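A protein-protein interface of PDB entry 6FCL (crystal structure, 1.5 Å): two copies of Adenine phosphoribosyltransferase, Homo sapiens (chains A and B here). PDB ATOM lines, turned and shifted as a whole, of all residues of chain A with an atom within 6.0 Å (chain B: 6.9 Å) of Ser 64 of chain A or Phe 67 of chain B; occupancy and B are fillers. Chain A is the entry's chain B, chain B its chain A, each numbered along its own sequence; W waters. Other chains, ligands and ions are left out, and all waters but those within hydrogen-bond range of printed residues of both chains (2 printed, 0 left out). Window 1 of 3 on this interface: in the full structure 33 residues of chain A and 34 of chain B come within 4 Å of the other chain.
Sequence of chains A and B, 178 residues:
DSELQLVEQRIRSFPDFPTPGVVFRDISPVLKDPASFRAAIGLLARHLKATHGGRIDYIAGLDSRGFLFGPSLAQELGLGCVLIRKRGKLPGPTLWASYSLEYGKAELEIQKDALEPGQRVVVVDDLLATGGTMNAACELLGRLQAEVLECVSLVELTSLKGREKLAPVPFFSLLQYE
The guanidinium group of Arg 85 of chain B lies within hydrogen-bond range of the side-chain hydroxyl of Ser 64 of chain A, 2.6 Å away.
O of Phe 67 of chain A sits close to O of Phe 67 of chain B (3.3 Å).
The side-chain carboxylate of Asp 63 of chain B lies within salt-bridge range of the guanidinium group of Arg 85 of chain B, 2.9 Å away.
The backbone NH (N) of Asp 63 of chain B sits at hydrogen-bond distance from the backbone carbonyl oxygen (O) of Ile 84 of chain B (3.0 Å).
The backbone NH of Phe 67 of chain A is in hydrogen-bond range of the backbone carbonyl oxygen of Leu 62 of chain A, 3.3 Å away.
The side-chain carboxylate (OD2) of Asp 63 of chain B sits at hydrogen-bond distance from the backbone NH (N) of Lys 86 of chain B.
The backbone carbonyl oxygen of Leu 62 of chain B sits at hydrogen-bond distance from the backbone NH of Phe 67 of chain B.
OD2 of Asp 63 of chain A is in hydrogen-bond range of N of Lys 86 of chain A, 3.0 Å away.
Asp 63 of chain A touches Ser 64 of chain B (OD1 to CB, 3.9 Å).
Asp 63 of chain B touches Ser 64 of chain A (OD1 to CB, 3.8 Å).
Ser 64 of chain A touches Phe 67 of chain B (O to CD2, 3.5 Å).
Arg 65 of chain A touches Arg 85 of chain B.
Phe 67 of chain A touches Ser 64 of chain B (CD2 to O, 3.5 Å).
Phe 67 of chain A touches Leu 68 of chain B.
Phe 67 of chain B touches Leu 68 of chain A.
Leu 68 of chain A touches Pro 71 of chain B.
Leu 83 of chain B touches Leu 68 of chain A.
CG of Pro 71 of chain A touches O of Leu 68 of chain B, 3.6 Å away.
Printed residues of chain B within 4 Å of Ser 64 of chain A: Asp 63 (3.8 Å), Phe 67 (3.5 Å) and Arg 85 (2.6 Å).
Printed residues of chain B within 4 Å of Arg 65 of chain A: Arg 85.
Of the printed residues of chain B, Pro 71 of chain A touches Leu 68 (3.6 Å).
Gly 66 of chain B touches none of the printed residues of chain A.
Of chain A, only Ser 64, Phe 67 and Leu 68 come within 4 Å of Phe 67 of chain B.
Of the printed residues of chain A, Pro 71 of chain B touches Leu 68.
Ser 72 of chain B touches none of the printed residues of chain A.
The nearest printed residue of chain B that does not touch Ser 64 of chain A is Ser 64 of chain B (4.2 Å).
Of the 22 printed residues of chain B, 7 touch a printed residue of chain A.
Hydrophobic or aromatic side chains of chain B within 4 Å of the printed part of chain A: Phe 67, Leu 68, Pro 71 and Leu 83.
Of the 11 printed residues of chain A, 6 touch a printed residue of chain B.
Hydrophobic or aromatic side chains of chain A that line the printed part of chain B: Phe 67, Leu 68 and Pro 71.
Among the printed residues, 12 pairs touch across the chains.
Among the printed residues, no Asp or Glu carboxylate lies within 4 Å of a Lys or Arg side-chain nitrogen of the other chain.
Asp 63 of chain A touches Ser 64 of chain B, and with the chains exchanged Ser 64 of chain A touches Asp 63 of chain B.
Ser 64 of chain A touches Phe 67 of chain B, and with the chains exchanged Phe 67 of chain A touches Ser 64 of chain B.
Phe 67 of chain B touches its own counterpart, Phe 67 of chain A.
Leu 68 of chain A touches Pro 71 of chain B, and with the chains exchanged Pro 71 of chain A touches Leu 68 of chain B.
11 positions are printed for both chains.
Water W2 lies within hydrogen-bond range of the backbone carbonyl oxygen (O) of Lys 89 of chain B (2.8 Å), the guanidinium group (NH1) of Arg 85 of chain B (3.2 Å) and the guanidinium group (NH1) of Arg 65 of chain A (3.4 Å).
Water W1 lies within hydrogen-bond range of the backbone carbonyl oxygen (O) of Lys 89 of chain B (2.9 Å) and the guanidinium group (NH1) of Arg 65 of chain A (3.4 Å).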
ATOM      1  N   LEU A  62      28.308   8.410 -11.092  1.00  0.00           N
ATOM      2  CA  LEU A  62      29.740   8.542 -11.366  1.00  0.00           C
ATOM      3  C   LEU A  62      30.048   9.377 -12.616  1.00  0.00           C
ATOM      4  O   LEU A  62      29.451   9.197 -13.681  1.00  0.00           O
ATOM      5  CB  LEU A  62      30.381   7.170 -11.517  1.00  0.00           C
ATOM      6  CG  LEU A  62      30.241   6.204 -10.346  1.00  0.00           C
ATOM      7  CD1 LEU A  62      31.216   5.042 -10.520  1.00  0.00           C
ATOM      8  CD2 LEU A  62      30.469   6.885  -9.008  1.00  0.00           C
ATOM      9  N   ASP A  63      30.956  10.326 -12.442  1.00  0.00           N
ATOM     10  CA  ASP A  63      31.461  11.200 -13.499  1.00  0.00           C
ATOM     11  C   ASP A  63      32.158  10.331 -14.542  1.00  0.00           C
ATOM     12  O   ASP A  63      33.011   9.533 -14.167  1.00  0.00           O
ATOM     13  CB  ASP A  63      32.511  12.107 -12.843  1.00  0.00           C
ATOM     14  CG  ASP A  63      32.803  13.374 -13.612  1.00  0.00           C
ATOM     15  OD1 ASP A  63      32.460  13.487 -14.815  1.00  0.00           O
ATOM     16  OD2 ASP A  63      33.404  14.288 -12.991  1.00  0.00           O
ATOM     17  N   SER A  64      31.832  10.462 -15.837  1.00  0.00           N
ATOM     18  CA  SER A  64      30.826  11.389 -16.339  1.00  0.00           C
ATOM     19  C   SER A  64      29.607  10.675 -16.923  1.00  0.00           C
ATOM     20  O   SER A  64      28.522  11.252 -16.978  1.00  0.00           O
ATOM     21  CB  SER A  64      31.429  12.262 -17.438  1.00  0.00           C
ATOM     22  OG  SER A  64      31.986  11.439 -18.443  1.00  0.00           O
ATOM     23  N   ARG A  65      29.774   9.443 -17.406  1.00  0.00           N
ATOM     24  CA  ARG A  65      28.655   8.762 -18.063  1.00  0.00           C
ATOM     25  C   ARG A  65      27.595   8.253 -17.090  1.00  0.00           C
ATOM     26  O   ARG A  65      26.437   8.052 -17.460  1.00  0.00           O
ATOM     27  CB  ARG A  65      29.144   7.671 -19.014  1.00  0.00           C
ATOM     28  CG  ARG A  65      29.900   8.269 -20.192  1.00  0.00           C
ATOM     29  CD  ARG A  65      29.988   7.346 -21.392  1.00  0.00           C
ATOM     30  NE  ARG A  65      30.541   6.035 -21.073  1.00  0.00           N
ATOM     31  CZ  ARG A  65      31.794   5.658 -21.313  1.00  0.00           C
ATOM     32  NH1 ARG A  65      32.666   6.510 -21.836  1.00  0.00           N
ATOM     33  NH2 ARG A  65      32.171   4.421 -21.022  1.00  0.00           N
ATOM     34  N   GLY A  66      27.965   8.103 -15.824  1.00  0.00           N
ATOM     35  CA  GLY A  66      26.999   7.776 -14.807  1.00  0.00           C
ATOM     36  C   GLY A  66      26.058   8.936 -14.534  1.00  0.00           C
ATOM     37  O   GLY A  66      24.922   8.723 -14.126  1.00  0.00           O
ATOM     38  N   PHE A  67      26.528  10.163 -14.777  1.00  0.00           N
ATOM     39  CA  PHE A  67      25.698  11.354 -14.672  1.00  0.00           C
ATOM     40  C   PHE A  67      24.490  11.293 -15.613  1.00  0.00           C
ATOM     41  O   PHE A  67      23.460  11.920 -15.350  1.00  0.00           O
ATOM     42  CB  PHE A  67      26.496  12.609 -15.023  1.00  0.00           C
ATOM     43  CG  PHE A  67      27.464  13.073 -13.962  1.00  0.00           C
ATOM     44  CD1 PHE A  67      27.682  12.359 -12.799  1.00  0.00           C
ATOM     45  CD2 PHE A  67      28.204  14.225 -14.187  1.00  0.00           C
ATOM     46  CE1 PHE A  67      28.571  12.826 -11.847  1.00  0.00           C
ATOM     47  CE2 PHE A  67      29.121  14.674 -13.253  1.00  0.00           C
ATOM     48  CZ  PHE A  67      29.302  13.968 -12.084  1.00  0.00           C
ATOM     49  N   LEU A  68      24.625  10.567 -16.721  1.00  0.00           N
ATOM     50  CA  LEU A  68      23.537  10.428 -17.682  1.00  0.00           C
ATOM     51  C   LEU A  68      22.377   9.602 -17.150  1.00  0.00           C
ATOM     52  O   LEU A  68      21.235   9.798 -17.582  1.00  0.00           O
ATOM     53  CB  LEU A  68      24.043   9.782 -18.964  1.00  0.00           C
ATOM     54  CG  LEU A  68      25.061  10.583 -19.770  1.00  0.00           C
ATOM     55  CD1 LEU A  68      25.758   9.700 -20.790  1.00  0.00           C
ATOM     56  CD2 LEU A  68      24.382  11.761 -20.449  1.00  0.00           C
ATOM     57  N   PHE A  69      22.658   8.741 -16.167  1.00  0.00           N
ATOM     58  CA  PHE A  69      21.642   7.822 -15.635  1.00  0.00           C
ATOM     59  C   PHE A  69      21.224   8.093 -14.190  1.00  0.00           C
ATOM     60  O   PHE A  69      20.069   7.859 -13.823  1.00  0.00           O
ATOM     61  CB  PHE A  69      22.127   6.387 -15.787  1.00  0.00           C
ATOM     62  CG  PHE A  69      22.370   6.012 -17.213  1.00  0.00           C
ATOM     63  CD1 PHE A  69      21.307   5.670 -18.035  1.00  0.00           C
ATOM     64  CD2 PHE A  69      23.645   6.071 -17.752  1.00  0.00           C
ATOM     65  CE1 PHE A  69      21.513   5.371 -19.369  1.00  0.00           C
ATOM     66  CE2 PHE A  69      23.850   5.782 -19.084  1.00  0.00           C
ATOM     67  CZ  PHE A  69      22.788   5.409 -19.884  1.00  0.00           C
ATOM     68  N   PRO A  71      20.555  10.877 -12.189  1.00  0.00           N
ATOM     69  CA  PRO A  71      19.424  11.714 -11.822  1.00  0.00           C
ATOM     70  C   PRO A  71      18.082  11.141 -12.265  1.00  0.00           C
ATOM     71  O   PRO A  71      17.129  11.174 -11.494  1.00  0.00           O
ATOM     72  CB  PRO A  71      19.730  13.055 -12.505  1.00  0.00           C
ATOM     73  CG  PRO A  71      21.218  13.078 -12.645  1.00  0.00           C
ATOM     74  CD  PRO A  71      21.633  11.653 -12.835  1.00  0.00           C
ATOM     75  N   LYS A  86      35.483  13.489 -10.995  1.00  0.00           N
ATOM     76  CA  LYS A  86      36.920  13.476 -11.196  1.00  0.00           C
ATOM     77  C   LYS A  86      37.507  14.567 -10.316  1.00  0.00           C
ATOM     78  O   LYS A  86      36.896  15.621 -10.122  1.00  0.00           O
ATOM     79  CB  LYS A  86      37.277  13.715 -12.667  1.00  0.00           C
ATOM     80  CG  LYS A  86      36.641  12.690 -13.587  1.00  0.00           C
ATOM     81  CD  LYS A  86      37.578  12.250 -14.698  1.00  0.00           C
ATOM     82  CE  LYS A  86      36.876  11.292 -15.649  1.00  0.00           C
ATOM     83  NZ  LYS A  86      36.100  10.253 -14.915  1.00  0.00           N
ATOM     84  N   ASP A 125      26.834   3.592 -12.753  1.00  0.00           N
ATOM     85  CA  ASP A 125      27.671   4.042 -13.877  1.00  0.00           C
ATOM     86  C   ASP A 125      27.133   3.346 -15.140  1.00  0.00           C
ATOM     87  O   ASP A 125      26.310   2.423 -15.049  1.00  0.00           O
ATOM     88  CB  ASP A 125      29.139   3.665 -13.621  1.00  0.00           C
ATOM     89  CG  ASP A 125      30.140   4.532 -14.398  1.00  0.00           C
ATOM     90  OD1 ASP A 125      29.736   5.419 -15.174  1.00  0.00           O
ATOM     91  OD2 ASP A 125      31.363   4.326 -14.219  1.00  0.00           O
ATOM     92  N   GLY B  61      23.106  17.497 -24.610  1.00  0.00           N
ATOM     93  CA  GLY B  61      23.701  17.728 -23.299  1.00  0.00           C
ATOM     94  C   GLY B  61      25.199  17.920 -23.392  1.00  0.00           C
ATOM     95  O   GLY B  61      25.889  17.156 -24.084  1.00  0.00           O
ATOM     96  N   LEU B  62      25.715  18.922 -22.678  1.00  0.00           N
ATOM     97  CA  LEU B  62      27.152  19.200 -22.669  1.00  0.00           C
ATOM     98  C   LEU B  62      27.885  18.505 -21.515  1.00  0.00           C
ATOM     99  O   LEU B  62      27.490  18.602 -20.344  1.00  0.00           O
ATOM    100  CB  LEU B  62      27.409  20.698 -22.561  1.00  0.00           C
ATOM    101  CG  LEU B  62      26.831  21.577 -23.649  1.00  0.00           C
ATOM    102  CD1 LEU B  62      27.522  22.941 -23.635  1.00  0.00           C
ATOM    103  CD2 LEU B  62      26.974  20.907 -25.004  1.00  0.00           C
ATOM    104  N   ASP B  63      28.936  17.778 -21.867  1.00  0.00           N
ATOM    105  CA  ASP B  63      29.864  17.162 -20.914  1.00  0.00           C
ATOM    106  C   ASP B  63      30.435  18.264 -20.018  1.00  0.00           C
ATOM    107  O   ASP B  63      30.908  19.262 -20.550  1.00  0.00           O
ATOM    108  CB  ASP B  63      31.006  16.547 -21.745  1.00  0.00           C
ATOM    109  CG  ASP B  63      31.801  15.477 -21.009  1.00  0.00           C
ATOM    110  OD1 ASP B  63      31.620  15.292 -19.787  1.00  0.00           O
ATOM    111  OD2 ASP B  63      32.615  14.803 -21.687  1.00  0.00           O
ATOM    112  N   SER B  64      30.449  18.115 -18.687  1.00  0.00           N
ATOM    113  CA  SER B  64      29.953  16.929 -17.994  1.00  0.00           C
ATOM    114  C   SER B  64      28.684  17.223 -17.186  1.00  0.00           C
ATOM    115  O   SER B  64      27.846  16.341 -16.971  1.00  0.00           O
ATOM    116  CB  SER B  64      31.034  16.413 -17.043  1.00  0.00           C
ATOM    117  OG  SER B  64      31.549  17.479 -16.267  1.00  0.00           O
ATOM    118  N   ARG B  65      28.560  18.447 -16.677  1.00  0.00           N
ATOM    119  CA  ARG B  65      27.411  18.774 -15.832  1.00  0.00           C
ATOM    120  C   ARG B  65      26.098  18.937 -16.608  1.00  0.00           C
ATOM    121  O   ARG B  65      25.016  18.835 -16.034  1.00  0.00           O
ATOM    122  CB  ARG B  65      27.702  19.990 -14.952  1.00  0.00           C
ATOM    123  CG  ARG B  65      28.615  19.692 -13.766  1.00  0.00           C
ATOM    124  CD  ARG B  65      28.852  20.939 -12.923  1.00  0.00           C
ATOM    125  NE  ARG B  65      30.154  21.544 -13.196  1.00  0.00           N
ATOM    126  CZ  ARG B  65      30.425  22.842 -13.104  1.00  0.00           C
ATOM    127  NH1 ARG B  65      29.456  23.721 -12.878  1.00  0.00           N
ATOM    128  NH2 ARG B  65      31.657  23.269 -13.342  1.00  0.00           N
ATOM    129  N   GLY B  66      26.189  19.150 -17.920  1.00  0.00           N
ATOM    130  CA  GLY B  66      25.001  19.164 -18.750  1.00  0.00           C
ATOM    131  C   GLY B  66      24.375  17.780 -18.853  1.00  0.00           C
ATOM    132  O   GLY B  66      23.183  17.630 -19.120  1.00  0.00           O
ATOM    133  N   PHE B  67      25.210  16.757 -18.724  1.00  0.00           N
ATOM    134  CA  PHE B  67      24.741  15.380 -18.695  1.00  0.00           C
ATOM    135  C   PHE B  67      23.753  15.132 -17.561  1.00  0.00           C
ATOM    136  O   PHE B  67      22.938  14.215 -17.641  1.00  0.00           O
ATOM    137  CB  PHE B  67      25.923  14.427 -18.509  1.00  0.00           C
ATOM    138  CG  PHE B  67      26.763  14.212 -19.741  1.00  0.00           C
ATOM    139  CD1 PHE B  67      26.568  14.942 -20.895  1.00  0.00           C
ATOM    140  CD2 PHE B  67      27.783  13.274 -19.707  1.00  0.00           C
ATOM    141  CE1 PHE B  67      27.370  14.723 -21.999  1.00  0.00           C
ATOM    142  CE2 PHE B  67      28.597  13.075 -20.793  1.00  0.00           C
ATOM    143  CZ  PHE B  67      28.381  13.794 -21.949  1.00  0.00           C
ATOM    144  N   LEU B  68      23.853  15.919 -16.493  1.00  0.00           N
ATOM    145  CA  LEU B  68      22.986  15.722 -15.331  1.00  0.00           C
ATOM    146  C   LEU B  68      21.558  16.163 -15.619  1.00  0.00           C
ATOM    147  O   LEU B  68      20.616  15.681 -14.987  1.00  0.00           O
ATOM    148  CB  LEU B  68      23.519  16.505 -14.145  1.00  0.00           C
ATOM    149  CG  LEU B  68      24.850  16.025 -13.589  1.00  0.00           C
ATOM    150  CD1 LEU B  68      25.468  17.098 -12.711  1.00  0.00           C
ATOM    151  CD2 LEU B  68      24.662  14.712 -12.844  1.00  0.00           C
ATOM    152  N   PHE B  69      21.396  17.046 -16.604  1.00  0.00           N
ATOM    153  CA  PHE B  69      20.089  17.635 -16.897  1.00  0.00           C
ATOM    154  C   PHE B  69      19.509  17.240 -18.257  1.00  0.00           C
ATOM    155  O   PHE B  69      18.293  17.138 -18.399  1.00  0.00           O
ATOM    156  CB  PHE B  69      20.177  19.151 -16.797  1.00  0.00           C
ATOM    157  CG  PHE B  69      20.537  19.630 -15.422  1.00  0.00           C
ATOM    158  CD1 PHE B  69      19.565  19.741 -14.444  1.00  0.00           C
ATOM    159  CD2 PHE B  69      21.854  19.919 -15.095  1.00  0.00           C
ATOM    160  CE1 PHE B  69      19.899  20.123 -13.153  1.00  0.00           C
ATOM    161  CE2 PHE B  69      22.181  20.319 -13.816  1.00  0.00           C
ATOM    162  CZ  PHE B  69      21.197  20.439 -12.852  1.00  0.00           C
ATOM    163  N   GLY B  70      20.380  17.001 -19.241  1.00  0.00           N
ATOM    164  CA  GLY B  70      19.935  16.716 -20.615  1.00  0.00           C
ATOM    165  C   GLY B  70      18.968  15.568 -20.744  1.00  0.00           C
ATOM    166  O   GLY B  70      17.895  15.731 -21.315  1.00  0.00           O
ATOM    167  N   PRO B  71      19.323  14.385 -20.211  1.00  0.00           N
ATOM    168  CA  PRO B  71      18.435  13.248 -20.395  1.00  0.00           C
ATOM    169  C   PRO B  71      17.081  13.429 -19.706  1.00  0.00           C
ATOM    170  O   PRO B  71      16.067  13.082 -20.281  1.00  0.00           O
ATOM    171  CB  PRO B  71      19.225  12.083 -19.778  1.00  0.00           C
ATOM    172  CG  PRO B  71      20.646  12.498 -19.933  1.00  0.00           C
ATOM    173  CD  PRO B  71      20.640  13.976 -19.689  1.00  0.00           C
ATOM    174  N   SER B  72      17.052  13.978 -18.496  1.00  0.00           N
ATOM    175  CA  SER B  72      15.777  14.216 -17.818  1.00  0.00           C
ATOM    176  C   SER B  72      14.934  15.253 -18.538  1.00  0.00           C
ATOM    177  O   SER B  72      13.722  15.107 -18.649  1.00  0.00           O
ATOM    178  CB  SER B  72      16.038  14.665 -16.381  1.00  0.00           C
ATOM    179  OG  SER B  72      16.569  13.583 -15.625  1.00  0.00           O
ATOM    180  N   CYS B  81      18.183  12.517 -26.390  1.00  0.00           N
ATOM    181  CA  CYS B  81      19.258  13.402 -25.979  1.00  0.00           C
ATOM    182  C   CYS B  81      20.532  12.947 -26.687  1.00  0.00           C
ATOM    183  O   CYS B  81      20.849  11.747 -26.679  1.00  0.00           O
ATOM    184  CB  CYS B  81      19.446  13.335 -24.455  1.00  0.00           C
ATOM    185  SG  CYS B  81      20.673  14.493 -23.816  1.00  0.00           S
ATOM    186  N   VAL B  82      21.197  13.880 -27.368  1.00  0.00           N
ATOM    187  CA  VAL B  82      22.496  13.619 -27.976  1.00  0.00           C
ATOM    188  C   VAL B  82      23.606  14.234 -27.110  1.00  0.00           C
ATOM    189  O   VAL B  82      23.351  15.094 -26.247  1.00  0.00           O
ATOM    190  CB  VAL B  82      22.587  14.097 -29.459  1.00  0.00           C
ATOM    191  CG1 VAL B  82      21.516  13.417 -30.310  1.00  0.00           C
ATOM    192  CG2 VAL B  82      22.495  15.607 -29.579  1.00  0.00           C
ATOM    193  N   LEU B  83      24.831  13.746 -27.289  1.00  0.00           N
ATOM    194  CA  LEU B  83      25.915  14.125 -26.383  1.00  0.00           C
ATOM    195  C   LEU B  83      27.000  14.890 -27.099  1.00  0.00           C
ATOM    196  O   LEU B  83      27.427  14.488 -28.168  1.00  0.00           O
ATOM    197  CB  LEU B  83      26.570  12.884 -25.786  1.00  0.00           C
ATOM    198  CG  LEU B  83      25.683  11.814 -25.174  1.00  0.00           C
ATOM    199  CD1 LEU B  83      26.567  10.694 -24.653  1.00  0.00           C
ATOM    200  CD2 LEU B  83      24.856  12.423 -24.066  1.00  0.00           C
ATOM    201  N   ILE B  84      27.472  15.958 -26.457  1.00  0.00           N
ATOM    202  CA  ILE B  84      28.666  16.660 -26.880  1.00  0.00           C
ATOM    203  C   ILE B  84      29.709  16.474 -25.789  1.00  0.00           C
ATOM    204  O   ILE B  84      29.460  16.782 -24.627  1.00  0.00           O
ATOM    205  CB  ILE B  84      28.383  18.147 -27.126  1.00  0.00           C
ATOM    206  CG1 ILE B  84      27.415  18.281 -28.314  1.00  0.00           C
ATOM    207  CG2 ILE B  84      29.684  18.901 -27.389  1.00  0.00           C
ATOM    208  CD1 ILE B  84      26.854  19.666 -28.502  1.00  0.00           C
ATOM    209  N   ARG B  85      30.857  15.917 -26.157  1.00  0.00           N
ATOM    210  CA  ARG B  85      31.841  15.477 -25.172  1.00  0.00           C
ATOM    211  C   ARG B  85      33.192  16.124 -25.307  1.00  0.00           C
ATOM    212  O   ARG B  85      33.511  16.718 -26.338  1.00  0.00           O
ATOM    213  CB  ARG B  85      32.041  13.970 -25.289  1.00  0.00           C
ATOM    214  CG  ARG B  85      30.801  13.156 -24.962  1.00  0.00           C
ATOM    215  CD  ARG B  85      31.183  11.912 -24.183  1.00  0.00           C
ATOM    216  NE  ARG B  85      31.827  12.279 -22.926  1.00  0.00           N
ATOM    217  CZ  ARG B  85      32.245  11.415 -22.008  1.00  0.00           C
ATOM    218  NH1 ARG B  85      32.115  10.110 -22.211  1.00  0.00           N
ATOM    219  NH2 ARG B  85      32.818  11.859 -20.898  1.00  0.00           N
ATOM    220  N   LYS B  86      33.983  16.013 -24.240  1.00  0.00           N
ATOM    221  CA  LYS B  86      35.389  16.395 -24.291  1.00  0.00           C
ATOM    222  C   LYS B  86      36.047  15.521 -25.344  1.00  0.00           C
ATOM    223  O   LYS B  86      35.727  14.338 -25.462  1.00  0.00           O
ATOM    224  CB  LYS B  86      36.058  16.157 -22.931  1.00  0.00           C
ATOM    225  CG  LYS B  86      35.483  17.015 -21.819  1.00  0.00           C
ATOM    226  CD  LYS B  86      35.608  18.494 -22.150  1.00  0.00           C
ATOM    227  CE  LYS B  86      34.653  19.334 -21.319  1.00  0.00           C
ATOM    228  NZ  LYS B  86      34.875  19.135 -19.861  1.00  0.00           N
ATOM    229  N   LYS B  89      36.776  11.060 -26.163  1.00  0.00           N
ATOM    230  CA  LYS B  89      35.898  10.157 -25.420  1.00  0.00           C
ATOM    231  C   LYS B  89      34.935   9.353 -26.295  1.00  0.00           C
ATOM    232  O   LYS B  89      34.476   8.283 -25.890  1.00  0.00           O
ATOM    233  CB  LYS B  89      35.071  10.944 -24.398  1.00  0.00           C
ATOM    234  CG  LYS B  89      35.879  11.777 -23.417  1.00  0.00           C
ATOM    235  CD  LYS B  89      36.777  10.922 -22.544  1.00  0.00           C
ATOM    236  CE  LYS B  89      37.190  11.687 -21.297  1.00  0.00           C
ATOM    237  NZ  LYS B  89      38.397  11.104 -20.651  1.00  0.00           N
ATOM    238  N   VAL B 124      21.771  22.147 -23.639  1.00  0.00           N
ATOM    239  CA  VAL B 124      21.669  22.382 -22.199  1.00  0.00           C
ATOM    240  C   VAL B 124      22.991  22.161 -21.466  1.00  0.00           C
ATOM    241  O   VAL B 124      23.734  21.216 -21.752  1.00  0.00           O
ATOM    242  CB  VAL B 124      20.563  21.543 -21.527  1.00  0.00           C
ATOM    243  CG1 VAL B 124      20.845  20.054 -21.616  1.00  0.00           C
ATOM    244  CG2 VAL B 124      20.353  21.976 -20.075  1.00  0.00           C
ATOM    245  N   ASP B 125      23.318  23.100 -20.584  1.00  0.00           N
ATOM    246  CA  ASP B 125      24.430  22.932 -19.642  1.00  0.00           C
ATOM    247  C   ASP B 125      23.936  23.478 -18.300  1.00  0.00           C
ATOM    248  O   ASP B 125      22.871  24.104 -18.226  1.00  0.00           O
ATOM    249  CB  ASP B 125      25.657  23.708 -20.140  1.00  0.00           C
ATOM    250  CG  ASP B 125      26.981  23.175 -19.578  1.00  0.00           C
ATOM    251  OD1 ASP B 125      26.983  22.259 -18.724  1.00  0.00           O
ATOM    252  OD2 ASP B 125      28.037  23.704 -20.001  1.00  0.00           O
ATOM    253  N   ASP B 126      24.683  23.255 -17.229  1.00  0.00           N
ATOM    254  CA  ASP B 126      24.233  23.744 -15.924  1.00  0.00           C
ATOM    255  C   ASP B 126      24.353  25.251 -15.783  1.00  0.00           C
ATOM    256  O   ASP B 126      23.469  25.886 -15.219  1.00  0.00           O
ATOM    257  CB  ASP B 126      24.942  23.019 -14.764  1.00  0.00           C
ATOM    258  CG  ASP B 126      26.425  23.358 -14.634  1.00  0.00           C
ATOM    259  OD1 ASP B 126      27.112  23.632 -15.631  1.00  0.00           O
ATOM    260  OD2 ASP B 126      26.928  23.279 -13.481  1.00  0.00           O
HETATM  261  O   HOH W   1      35.575   7.235 -23.394  1.00  0.00           O
HETATM  262  O   HOH W   2      31.911   8.181 -24.704  1.00  0.00           O
